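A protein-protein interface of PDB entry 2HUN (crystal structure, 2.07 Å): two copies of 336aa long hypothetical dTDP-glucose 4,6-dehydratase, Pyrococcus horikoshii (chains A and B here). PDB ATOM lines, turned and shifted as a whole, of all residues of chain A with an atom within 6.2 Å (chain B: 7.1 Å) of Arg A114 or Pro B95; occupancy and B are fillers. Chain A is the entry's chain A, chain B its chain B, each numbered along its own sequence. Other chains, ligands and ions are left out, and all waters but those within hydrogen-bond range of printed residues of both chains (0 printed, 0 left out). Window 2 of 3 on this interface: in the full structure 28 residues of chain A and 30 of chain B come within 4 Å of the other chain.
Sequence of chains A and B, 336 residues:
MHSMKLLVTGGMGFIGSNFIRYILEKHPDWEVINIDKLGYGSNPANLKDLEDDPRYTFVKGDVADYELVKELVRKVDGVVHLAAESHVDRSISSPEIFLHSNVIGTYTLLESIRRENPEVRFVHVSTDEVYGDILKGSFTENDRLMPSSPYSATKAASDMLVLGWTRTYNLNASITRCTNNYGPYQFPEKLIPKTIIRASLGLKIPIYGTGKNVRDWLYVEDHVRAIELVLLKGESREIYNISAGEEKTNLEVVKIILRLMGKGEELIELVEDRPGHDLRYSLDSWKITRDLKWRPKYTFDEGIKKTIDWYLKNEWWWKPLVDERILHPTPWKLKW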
ATOM      1  N   TYR A 107      16.549  13.295   6.480  1.00  0.00           N
ATOM      2  CA  TYR A 107      15.547  13.304   5.413  1.00  0.00           C
ATOM      3  C   TYR A 107      16.105  14.039   4.191  1.00  0.00           C
ATOM      4  O   TYR A 107      16.026  13.547   3.064  1.00  0.00           O
ATOM      5  CB  TYR A 107      14.286  14.029   5.895  1.00  0.00           C
ATOM      6  CG  TYR A 107      13.315  14.421   4.794  1.00  0.00           C
ATOM      7  CD1 TYR A 107      12.456  13.481   4.217  1.00  0.00           C
ATOM      8  CD2 TYR A 107      13.256  15.737   4.330  1.00  0.00           C
ATOM      9  CE1 TYR A 107      11.561  13.843   3.206  1.00  0.00           C
ATOM     10  CE2 TYR A 107      12.366  16.111   3.317  1.00  0.00           C
ATOM     11  CZ  TYR A 107      11.521  15.159   2.762  1.00  0.00           C
ATOM     12  OH  TYR A 107      10.629  15.523   1.774  1.00  0.00           O
ATOM     13  N   LEU A 109      19.206  14.647   3.380  1.00  0.00           N
ATOM     14  CA  LEU A 109      20.311  13.911   2.792  1.00  0.00           C
ATOM     15  C   LEU A 109      19.751  12.780   1.928  1.00  0.00           C
ATOM     16  O   LEU A 109      20.223  12.552   0.813  1.00  0.00           O
ATOM     17  CB  LEU A 109      21.204  13.336   3.895  1.00  0.00           C
ATOM     18  CG  LEU A 109      22.612  12.917   3.474  1.00  0.00           C
ATOM     19  CD1 LEU A 109      23.392  14.159   3.054  1.00  0.00           C
ATOM     20  CD2 LEU A 109      23.315  12.214   4.629  1.00  0.00           C
ATOM     21  N   LEU A 110      18.744  12.078   2.444  1.00  0.00           N
ATOM     22  CA  LEU A 110      18.123  10.977   1.706  1.00  0.00           C
ATOM     23  C   LEU A 110      17.493  11.498   0.414  1.00  0.00           C
ATOM     24  O   LEU A 110      17.618  10.884  -0.643  1.00  0.00           O
ATOM     25  CB  LEU A 110      17.065  10.277   2.576  1.00  0.00           C
ATOM     26  CG  LEU A 110      17.622   9.394   3.705  1.00  0.00           C
ATOM     27  CD1 LEU A 110      16.509   8.944   4.648  1.00  0.00           C
ATOM     28  CD2 LEU A 110      18.331   8.192   3.091  1.00  0.00           C
ATOM     29  N   GLU A 111      16.814  12.634   0.497  1.00  0.00           N
ATOM     30  CA  GLU A 111      16.190  13.203  -0.689  1.00  0.00           C
ATOM     31  C   GLU A 111      17.233  13.587  -1.727  1.00  0.00           C
ATOM     32  O   GLU A 111      17.068  13.295  -2.910  1.00  0.00           O
ATOM     33  CB  GLU A 111      15.341  14.421  -0.320  1.00  0.00           C
ATOM     34  CG  GLU A 111      13.939  14.074   0.184  1.00  0.00           C
ATOM     35  CD  GLU A 111      13.093  13.370  -0.872  1.00  0.00           C
ATOM     36  OE1 GLU A 111      13.176  12.130  -0.999  1.00  0.00           O
ATOM     37  OE2 GLU A 111      12.350  14.067  -1.589  1.00  0.00           O
ATOM     38  N   SER A 112      18.315  14.228  -1.292  1.00  0.00           N
ATOM     39  CA  SER A 112      19.359  14.629  -2.225  1.00  0.00           C
ATOM     40  C   SER A 112      19.956  13.392  -2.883  1.00  0.00           C
ATOM     41  O   SER A 112      20.273  13.399  -4.074  1.00  0.00           O
ATOM     42  CB  SER A 112      20.456  15.423  -1.502  1.00  0.00           C
ATOM     43  OG  SER A 112      21.230  14.590  -0.659  1.00  0.00           O
ATOM     44  N   ILE A 113      20.101  12.321  -2.110  1.00  0.00           N
ATOM     45  CA  ILE A 113      20.654  11.092  -2.653  1.00  0.00           C
ATOM     46  C   ILE A 113      19.750  10.450  -3.708  1.00  0.00           C
ATOM     47  O   ILE A 113      20.223  10.102  -4.794  1.00  0.00           O
ATOM     48  CB  ILE A 113      20.941  10.065  -1.535  1.00  0.00           C
ATOM     49  CG1 ILE A 113      22.171  10.510  -0.735  1.00  0.00           C
ATOM     50  CG2 ILE A 113      21.150   8.678  -2.139  1.00  0.00           C
ATOM     51  CD1 ILE A 113      22.462   9.658   0.492  1.00  0.00           C
ATOM     52  N   ARG A 114      18.457  10.305  -3.413  1.00  0.00           N
ATOM     53  CA  ARG A 114      17.547   9.676  -4.368  1.00  0.00           C
ATOM     54  C   ARG A 114      17.184  10.586  -5.541  1.00  0.00           C
ATOM     55  O   ARG A 114      16.842  10.103  -6.617  1.00  0.00           O
ATOM     56  CB  ARG A 114      16.270   9.175  -3.664  1.00  0.00           C
ATOM     57  CG  ARG A 114      15.285  10.246  -3.186  1.00  0.00           C
ATOM     58  CD  ARG A 114      14.220  10.560  -4.242  1.00  0.00           C
ATOM     59  NE  ARG A 114      13.224  11.502  -3.734  1.00  0.00           N
ATOM     60  CZ  ARG A 114      12.163  11.927  -4.416  1.00  0.00           C
ATOM     61  NH1 ARG A 114      11.942  11.493  -5.652  1.00  0.00           N
ATOM     62  NH2 ARG A 114      11.322  12.795  -3.861  1.00  0.00           N
ATOM     63  N   ARG A 115      17.268  11.896  -5.342  1.00  0.00           N
ATOM     64  CA  ARG A 115      16.947  12.829  -6.417  1.00  0.00           C
ATOM     65  C   ARG A 115      18.144  13.081  -7.334  1.00  0.00           C
ATOM     66  O   ARG A 115      17.979  13.223  -8.544  1.00  0.00           O
ATOM     67  CB  ARG A 115      16.454  14.164  -5.841  1.00  0.00           C
ATOM     68  CG  ARG A 115      15.110  14.077  -5.149  1.00  0.00           C
ATOM     69  CD  ARG A 115      14.717  15.395  -4.492  1.00  0.00           C
ATOM     70  NE  ARG A 115      14.747  16.513  -5.433  1.00  0.00           N
ATOM     71  CZ  ARG A 115      14.295  17.736  -5.164  1.00  0.00           C
ATOM     72  NH1 ARG A 115      13.763  18.012  -3.978  1.00  0.00           N
ATOM     73  NH2 ARG A 115      14.389  18.694  -6.078  1.00  0.00           N
ATOM     74  N   GLU A 116      19.347  13.110  -6.767  1.00  0.00           N
ATOM     75  CA  GLU A 116      20.558  13.384  -7.549  1.00  0.00           C
ATOM     76  C   GLU A 116      21.476  12.213  -7.890  1.00  0.00           C
ATOM     77  O   GLU A 116      21.993  12.140  -9.004  1.00  0.00           O
ATOM     78  CB  GLU A 116      21.410  14.434  -6.837  1.00  0.00           C
ATOM     79  CG  GLU A 116      20.782  15.809  -6.704  1.00  0.00           C
ATOM     80  CD  GLU A 116      20.761  16.578  -8.012  1.00  0.00           C
ATOM     81  OE1 GLU A 116      21.379  16.110  -8.992  1.00  0.00           O
ATOM     82  OE2 GLU A 116      20.136  17.657  -8.053  1.00  0.00           O
ATOM     83  N   ASN A 117      21.691  11.302  -6.945  1.00  0.00           N
ATOM     84  CA  ASN A 117      22.617  10.206  -7.185  1.00  0.00           C
ATOM     85  C   ASN A 117      22.281   8.952  -6.376  1.00  0.00           C
ATOM     86  O   ASN A 117      22.974   8.614  -5.416  1.00  0.00           O
ATOM     87  CB  ASN A 117      24.024  10.685  -6.830  1.00  0.00           C
ATOM     88  CG  ASN A 117      25.102   9.699  -7.226  1.00  0.00           C
ATOM     89  OD1 ASN A 117      24.907   8.894  -8.135  1.00  0.00           O
ATOM     90  ND2 ASN A 117      26.237   9.744  -6.539  1.00  0.00           N
ATOM     91  N   PRO A 118      21.227   8.229  -6.777  1.00  0.00           N
ATOM     92  CA  PRO A 118      20.802   7.013  -6.078  1.00  0.00           C
ATOM     93  C   PRO A 118      21.824   5.880  -5.983  1.00  0.00           C
ATOM     94  O   PRO A 118      21.626   4.934  -5.223  1.00  0.00           O
ATOM     95  CB  PRO A 118      19.538   6.604  -6.836  1.00  0.00           C
ATOM     96  CG  PRO A 118      19.794   7.110  -8.221  1.00  0.00           C
ATOM     97  CD  PRO A 118      20.383   8.476  -7.960  1.00  0.00           C
ATOM     98  N   TRP A 165      13.451   4.840   2.662  1.00  0.00           N
ATOM     99  CA  TRP A 165      13.950   5.435   1.423  1.00  0.00           C
ATOM    100  C   TRP A 165      14.821   4.452   0.642  1.00  0.00           C
ATOM    101  O   TRP A 165      14.761   4.391  -0.585  1.00  0.00           O
ATOM    102  CB  TRP A 165      14.745   6.705   1.735  1.00  0.00           C
ATOM    103  CG  TRP A 165      13.976   7.990   1.519  1.00  0.00           C
ATOM    104  CD1 TRP A 165      14.232   8.944   0.577  1.00  0.00           C
ATOM    105  CD2 TRP A 165      12.859   8.471   2.280  1.00  0.00           C
ATOM    106  NE1 TRP A 165      13.353   9.990   0.704  1.00  0.00           N
ATOM    107  CE2 TRP A 165      12.498   9.728   1.742  1.00  0.00           C
ATOM    108  CE3 TRP A 165      12.129   7.965   3.366  1.00  0.00           C
ATOM    109  CZ2 TRP A 165      11.440  10.490   2.253  1.00  0.00           C
ATOM    110  CZ3 TRP A 165      11.076   8.721   3.874  1.00  0.00           C
ATOM    111  CH2 TRP A 165      10.742   9.972   3.315  1.00  0.00           C
ATOM    112  N   TYR A 169      13.527   3.745  -3.132  1.00  0.00           N
ATOM    113  CA  TYR A 169      14.311   4.192  -4.277  1.00  0.00           C
ATOM    114  C   TYR A 169      15.530   3.342  -4.606  1.00  0.00           C
ATOM    115  O   TYR A 169      16.430   3.784  -5.322  1.00  0.00           O
ATOM    116  CB  TYR A 169      14.725   5.643  -4.040  1.00  0.00           C
ATOM    117  CG  TYR A 169      13.541   6.541  -3.753  1.00  0.00           C
ATOM    118  CD1 TYR A 169      12.645   6.887  -4.761  1.00  0.00           C
ATOM    119  CD2 TYR A 169      13.293   7.011  -2.462  1.00  0.00           C
ATOM    120  CE1 TYR A 169      11.530   7.677  -4.493  1.00  0.00           C
ATOM    121  CE2 TYR A 169      12.181   7.802  -2.183  1.00  0.00           C
ATOM    122  CZ  TYR A 169      11.303   8.129  -3.203  1.00  0.00           C
ATOM    123  OH  TYR A 169      10.189   8.895  -2.931  1.00  0.00           O
ATOM    124  N   LEU A 171      18.218   2.422  -2.942  1.00  0.00           N
ATOM    125  CA  LEU A 171      19.491   3.030  -2.604  1.00  0.00           C
ATOM    126  C   LEU A 171      20.483   1.975  -2.114  1.00  0.00           C
ATOM    127  O   LEU A 171      20.113   0.827  -1.860  1.00  0.00           O
ATOM    128  CB  LEU A 171      19.281   4.085  -1.519  1.00  0.00           C
ATOM    129  CG  LEU A 171      18.216   5.142  -1.823  1.00  0.00           C
ATOM    130  CD1 LEU A 171      18.170   6.144  -0.690  1.00  0.00           C
ATOM    131  CD2 LEU A 171      18.529   5.841  -3.138  1.00  0.00           C
ATOM    132  N   ARG B  90       1.261   7.704  -3.524  1.00  0.00           N
ATOM    133  CA  ARG B  90       1.507   9.136  -3.446  1.00  0.00           C
ATOM    134  C   ARG B  90       2.775   9.404  -2.635  1.00  0.00           C
ATOM    135  O   ARG B  90       3.487  10.368  -2.904  1.00  0.00           O
ATOM    136  CB  ARG B  90       0.323   9.850  -2.793  1.00  0.00           C
ATOM    137  CG  ARG B  90      -0.896  10.006  -3.683  1.00  0.00           C
ATOM    138  CD  ARG B  90      -2.128  10.254  -2.825  1.00  0.00           C
ATOM    139  NE  ARG B  90      -1.884  11.252  -1.783  1.00  0.00           N
ATOM    140  CZ  ARG B  90      -1.969  12.568  -1.959  1.00  0.00           C
ATOM    141  NH1 ARG B  90      -2.300  13.061  -3.145  1.00  0.00           N
ATOM    142  NH2 ARG B  90      -1.730  13.395  -0.948  1.00  0.00           N
ATOM    143  N   SER B  91       3.060   8.543  -1.655  1.00  0.00           N
ATOM    144  CA  SER B  91       4.245   8.717  -0.809  1.00  0.00           C
ATOM    145  C   SER B  91       5.536   8.506  -1.598  1.00  0.00           C
ATOM    146  O   SER B  91       6.553   9.148  -1.327  1.00  0.00           O
ATOM    147  CB  SER B  91       4.203   7.761   0.402  1.00  0.00           C
ATOM    148  OG  SER B  91       4.645   6.446   0.084  1.00  0.00           O
ATOM    149  N   ILE B  92       5.505   7.604  -2.574  1.00  0.00           N
ATOM    150  CA  ILE B  92       6.693   7.347  -3.390  1.00  0.00           C
ATOM    151  C   ILE B  92       6.887   8.515  -4.365  1.00  0.00           C
ATOM    152  O   ILE B  92       8.002   8.988  -4.582  1.00  0.00           O
ATOM    153  CB  ILE B  92       6.550   6.023  -4.189  1.00  0.00           C
ATOM    154  CG1 ILE B  92       6.438   4.842  -3.217  1.00  0.00           C
ATOM    155  CG2 ILE B  92       7.752   5.835  -5.121  1.00  0.00           C
ATOM    156  CD1 ILE B  92       6.133   3.510  -3.888  1.00  0.00           C
ATOM    157  N   SER B  93       5.785   8.986  -4.926  1.00  0.00           N
ATOM    158  CA  SER B  93       5.806  10.092  -5.873  1.00  0.00           C
ATOM    159  C   SER B  93       6.263  11.398  -5.219  1.00  0.00           C
ATOM    160  O   SER B  93       7.090  12.118  -5.771  1.00  0.00           O
ATOM    161  CB  SER B  93       4.411  10.263  -6.479  1.00  0.00           C
ATOM    162  OG  SER B  93       4.386  11.298  -7.441  1.00  0.00           O
ATOM    163  N   SER B  94       5.728  11.698  -4.041  1.00  0.00           N
ATOM    164  CA  SER B  94       6.095  12.920  -3.334  1.00  0.00           C
ATOM    165  C   SER B  94       6.032  12.731  -1.821  1.00  0.00           C
ATOM    166  O   SER B  94       5.021  13.031  -1.183  1.00  0.00           O
ATOM    167  CB  SER B  94       5.170  14.061  -3.746  1.00  0.00           C
ATOM    168  OG  SER B  94       5.615  15.274  -3.173  1.00  0.00           O
ATOM    169  N   PRO B  95       7.135  12.251  -1.222  1.00  0.00           N
ATOM    170  CA  PRO B  95       7.242  12.002   0.220  1.00  0.00           C
ATOM    171  C   PRO B  95       7.170  13.224   1.138  1.00  0.00           C
ATOM    172  O   PRO B  95       6.903  13.088   2.331  1.00  0.00           O
ATOM    173  CB  PRO B  95       8.580  11.276   0.338  1.00  0.00           C
ATOM    174  CG  PRO B  95       9.393  11.935  -0.731  1.00  0.00           C
ATOM    175  CD  PRO B  95       8.422  11.982  -1.894  1.00  0.00           C
ATOM    176  N   GLU B  96       7.397  14.416   0.596  1.00  0.00           N
ATOM    177  CA  GLU B  96       7.365  15.613   1.427  1.00  0.00           C
ATOM    178  C   GLU B  96       6.093  15.771   2.263  1.00  0.00           C
ATOM    179  O   GLU B  96       6.172  16.007   3.464  1.00  0.00           O
ATOM    180  CB  GLU B  96       7.570  16.867   0.577  1.00  0.00           C
ATOM    181  CG  GLU B  96       7.381  18.141   1.368  1.00  0.00           C
ATOM    182  CD  GLU B  96       7.502  19.380   0.514  1.00  0.00           C
ATOM    183  OE1 GLU B  96       7.053  19.342  -0.652  1.00  0.00           O
ATOM    184  OE2 GLU B  96       8.031  20.393   1.014  1.00  0.00           O
ATOM    185  N   ILE B  97       4.926  15.648   1.639  1.00  0.00           N
ATOM    186  CA  ILE B  97       3.675  15.796   2.378  1.00  0.00           C
ATOM    187  C   ILE B  97       3.560  14.735   3.471  1.00  0.00           C
ATOM    188  O   ILE B  97       2.881  14.940   4.481  1.00  0.00           O
ATOM    189  CB  ILE B  97       2.441  15.705   1.441  1.00  0.00           C
ATOM    190  CG1 ILE B  97       1.179  16.132   2.192  1.00  0.00           C
ATOM    191  CG2 ILE B  97       2.262  14.292   0.929  1.00  0.00           C
ATOM    192  CD1 ILE B  97       1.008  17.624   2.325  1.00  0.00           C
ATOM    193  N   PHE B  98       4.225  13.602   3.272  1.00  0.00           N
ATOM    194  CA  PHE B  98       4.184  12.531   4.259  1.00  0.00           C
ATOM    195  C   PHE B  98       5.085  12.847   5.448  1.00  0.00           C
ATOM    196  O   PHE B  98       4.724  12.572   6.587  1.00  0.00           O
ATOM    197  CB  PHE B  98       4.550  11.203   3.596  1.00  0.00           C
ATOM    198  CG  PHE B  98       3.453  10.667   2.718  1.00  0.00           C
ATOM    199  CD1 PHE B  98       3.200  11.240   1.473  1.00  0.00           C
ATOM    200  CD2 PHE B  98       2.617   9.654   3.170  1.00  0.00           C
ATOM    201  CE1 PHE B  98       2.127  10.818   0.694  1.00  0.00           C
ATOM    202  CE2 PHE B  98       1.541   9.224   2.400  1.00  0.00           C
ATOM    203  CZ  PHE B  98       1.295   9.810   1.156  1.00  0.00           C
ATOM    204  N   LEU B  99       6.245  13.442   5.186  1.00  0.00           N
ATOM    205  CA  LEU B  99       7.148  13.828   6.272  1.00  0.00           C
ATOM    206  C   LEU B  99       6.406  14.852   7.136  1.00  0.00           C
ATOM    207  O   LEU B  99       6.379  14.755   8.364  1.00  0.00           O
ATOM    208  CB  LEU B  99       8.424  14.472   5.715  1.00  0.00           C
ATOM    209  CG  LEU B  99       9.382  15.039   6.771  1.00  0.00           C
ATOM    210  CD1 LEU B  99      10.057  13.891   7.500  1.00  0.00           C
ATOM    211  CD2 LEU B  99      10.428  15.928   6.119  1.00  0.00           C
ATOM    212  N   HIS B 100       5.798  15.832   6.475  1.00  0.00           N
ATOM    213  CA  HIS B 100       5.057  16.891   7.162  1.00  0.00           C
ATOM    214  C   HIS B 100       3.894  16.394   8.027  1.00  0.00           C
ATOM    215  O   HIS B 100       3.891  16.574   9.243  1.00  0.00           O
ATOM    216  CB  HIS B 100       4.518  17.897   6.144  1.00  0.00           C
ATOM    217  CG  HIS B 100       3.670  18.969   6.752  1.00  0.00           C
ATOM    218  ND1 HIS B 100       4.205  20.065   7.396  1.00  0.00           N
ATOM    219  CD2 HIS B 100       2.325  19.101   6.837  1.00  0.00           C
ATOM    220  CE1 HIS B 100       3.226  20.826   7.852  1.00  0.00           C
ATOM    221  NE2 HIS B 100       2.075  20.264   7.526  1.00  0.00           N
ATOM    222  N   SER B 101       2.891  15.784   7.401  1.00  0.00           N
ATOM    223  CA  SER B 101       1.741  15.290   8.151  1.00  0.00           C
ATOM    224  C   SER B 101       2.071  14.199   9.165  1.00  0.00           C
ATOM    225  O   SER B 101       1.682  14.285  10.332  1.00  0.00           O
ATOM    226  CB  SER B 101       0.666  14.757   7.198  1.00  0.00           C
ATOM    227  OG  SER B 101      -0.050  15.816   6.583  1.00  0.00           O
ATOM    228  N   PRO B 150       7.757   5.505   1.722  1.00  0.00           N
ATOM    229  CA  PRO B 150       7.863   6.740   2.500  1.00  0.00           C
ATOM    230  C   PRO B 150       6.706   6.830   3.482  1.00  0.00           C
ATOM    231  O   PRO B 150       6.855   7.335   4.604  1.00  0.00           O
ATOM    232  CB  PRO B 150       7.815   7.822   1.424  1.00  0.00           C
ATOM    233  CG  PRO B 150       8.531   7.161   0.282  1.00  0.00           C
ATOM    234  CD  PRO B 150       7.890   5.787   0.282  1.00  0.00           C
ATOM    235  N   TYR B 151       5.550   6.337   3.053  1.00  0.00           N
ATOM    236  CA  TYR B 151       4.370   6.342   3.903  1.00  0.00           C
ATOM    237  C   TYR B 151       4.645   5.565   5.188  1.00  0.00           C
ATOM    238  O   TYR B 151       4.494   6.103   6.279  1.00  0.00           O
ATOM    239  CB  TYR B 151       3.172   5.704   3.187  1.00  0.00           C
ATOM    240  CG  TYR B 151       2.067   5.270   4.139  1.00  0.00           C
ATOM    241  CD1 TYR B 151       1.435   6.195   4.974  1.00  0.00           C
ATOM    242  CD2 TYR B 151       1.694   3.928   4.241  1.00  0.00           C
ATOM    243  CE1 TYR B 151       0.463   5.794   5.893  1.00  0.00           C
ATOM    244  CE2 TYR B 151       0.717   3.514   5.158  1.00  0.00           C
ATOM    245  CZ  TYR B 151       0.109   4.451   5.980  1.00  0.00           C
ATOM    246  OH  TYR B 151      -0.840   4.047   6.893  1.00  0.00           O
ATOM    247  N   THR B 154       7.606   7.122   7.389  1.00  0.00           N
ATOM    248  CA  THR B 154       7.269   8.303   8.171  1.00  0.00           C
ATOM    249  C   THR B 154       6.304   7.911   9.286  1.00  0.00           C
ATOM    250  O   THR B 154       6.322   8.510  10.357  1.00  0.00           O
ATOM    251  CB  THR B 154       6.660   9.432   7.290  1.00  0.00           C
ATOM    252  OG1 THR B 154       5.507   8.945   6.600  1.00  0.00           O
ATOM    253  CG2 THR B 154       7.688   9.921   6.262  1.00  0.00           C
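O of Ile B92 lies within hydrogen-bond range of OH of Tyr A169.
The indole nitrogen of Trp A165 sits at hydrogen-bond distance from the side-chain carboxylate of Glu A111, at 2.7 Å.
The side-chain hydroxyl of Ser B91 is in hydrogen-bond range of the backbone NH of Tyr B151.
The side-chain carboxylate of Glu A111 is in salt-bridge range of the guanidinium group of Arg A114.
Tyr A107 touches Glu B96.
Leu B99 touches Tyr A107.
OE2 of Glu A111 touches CG of Pro B95, at 3.7 Å.
Arg A114 touches Pro B95.
Pro B95 touches Trp A165 (CB to CZ2, 3.5 Å).
O of Ser B91 touches OH of Tyr A169, 3.98 Å away.
Tyr A169 touches Pro B95.
Arg A114 touches just one residue of chain B: Pro B95.
Of the printed residues of chain A, Ser B91 touches Tyr A169 (3.98 Å).
Printed residues of chain A within 4 Å of Ile B92: Tyr A169.
Pro B95 touches four residues of chain A.
Thr B154 touches none of the printed residues of chain A.
The nearest residue of chain B that does not touch Arg A114 is Ser B93 (4.7 Å).
The nearest residue of chain A that does not touch Pro B95 is Tyr A107 (4.2 Å).
The nearest printed residue of chain B that does not touch Tyr A107 is Pro B95 (4.2 Å).
Printed residues of chain A that touch a printed residue of chain B: Tyr A107, Glu A111, Arg A114, Trp A165 and Tyr A169.
Hydrophobic or aromatic side chains of chain A that line the printed part of chain B: Tyr A107, Trp A165 and Tyr A169.
Hydrophobic or aromatic side chains of chain B within 4 Å of the printed part of chain A: Pro B95 and Leu B99.
Among the printed residues, no Asp or Glu carboxylate lies within 4 Å of a Lys or Arg side-chain nitrogen of the other chain.
No position is printed for both chains.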
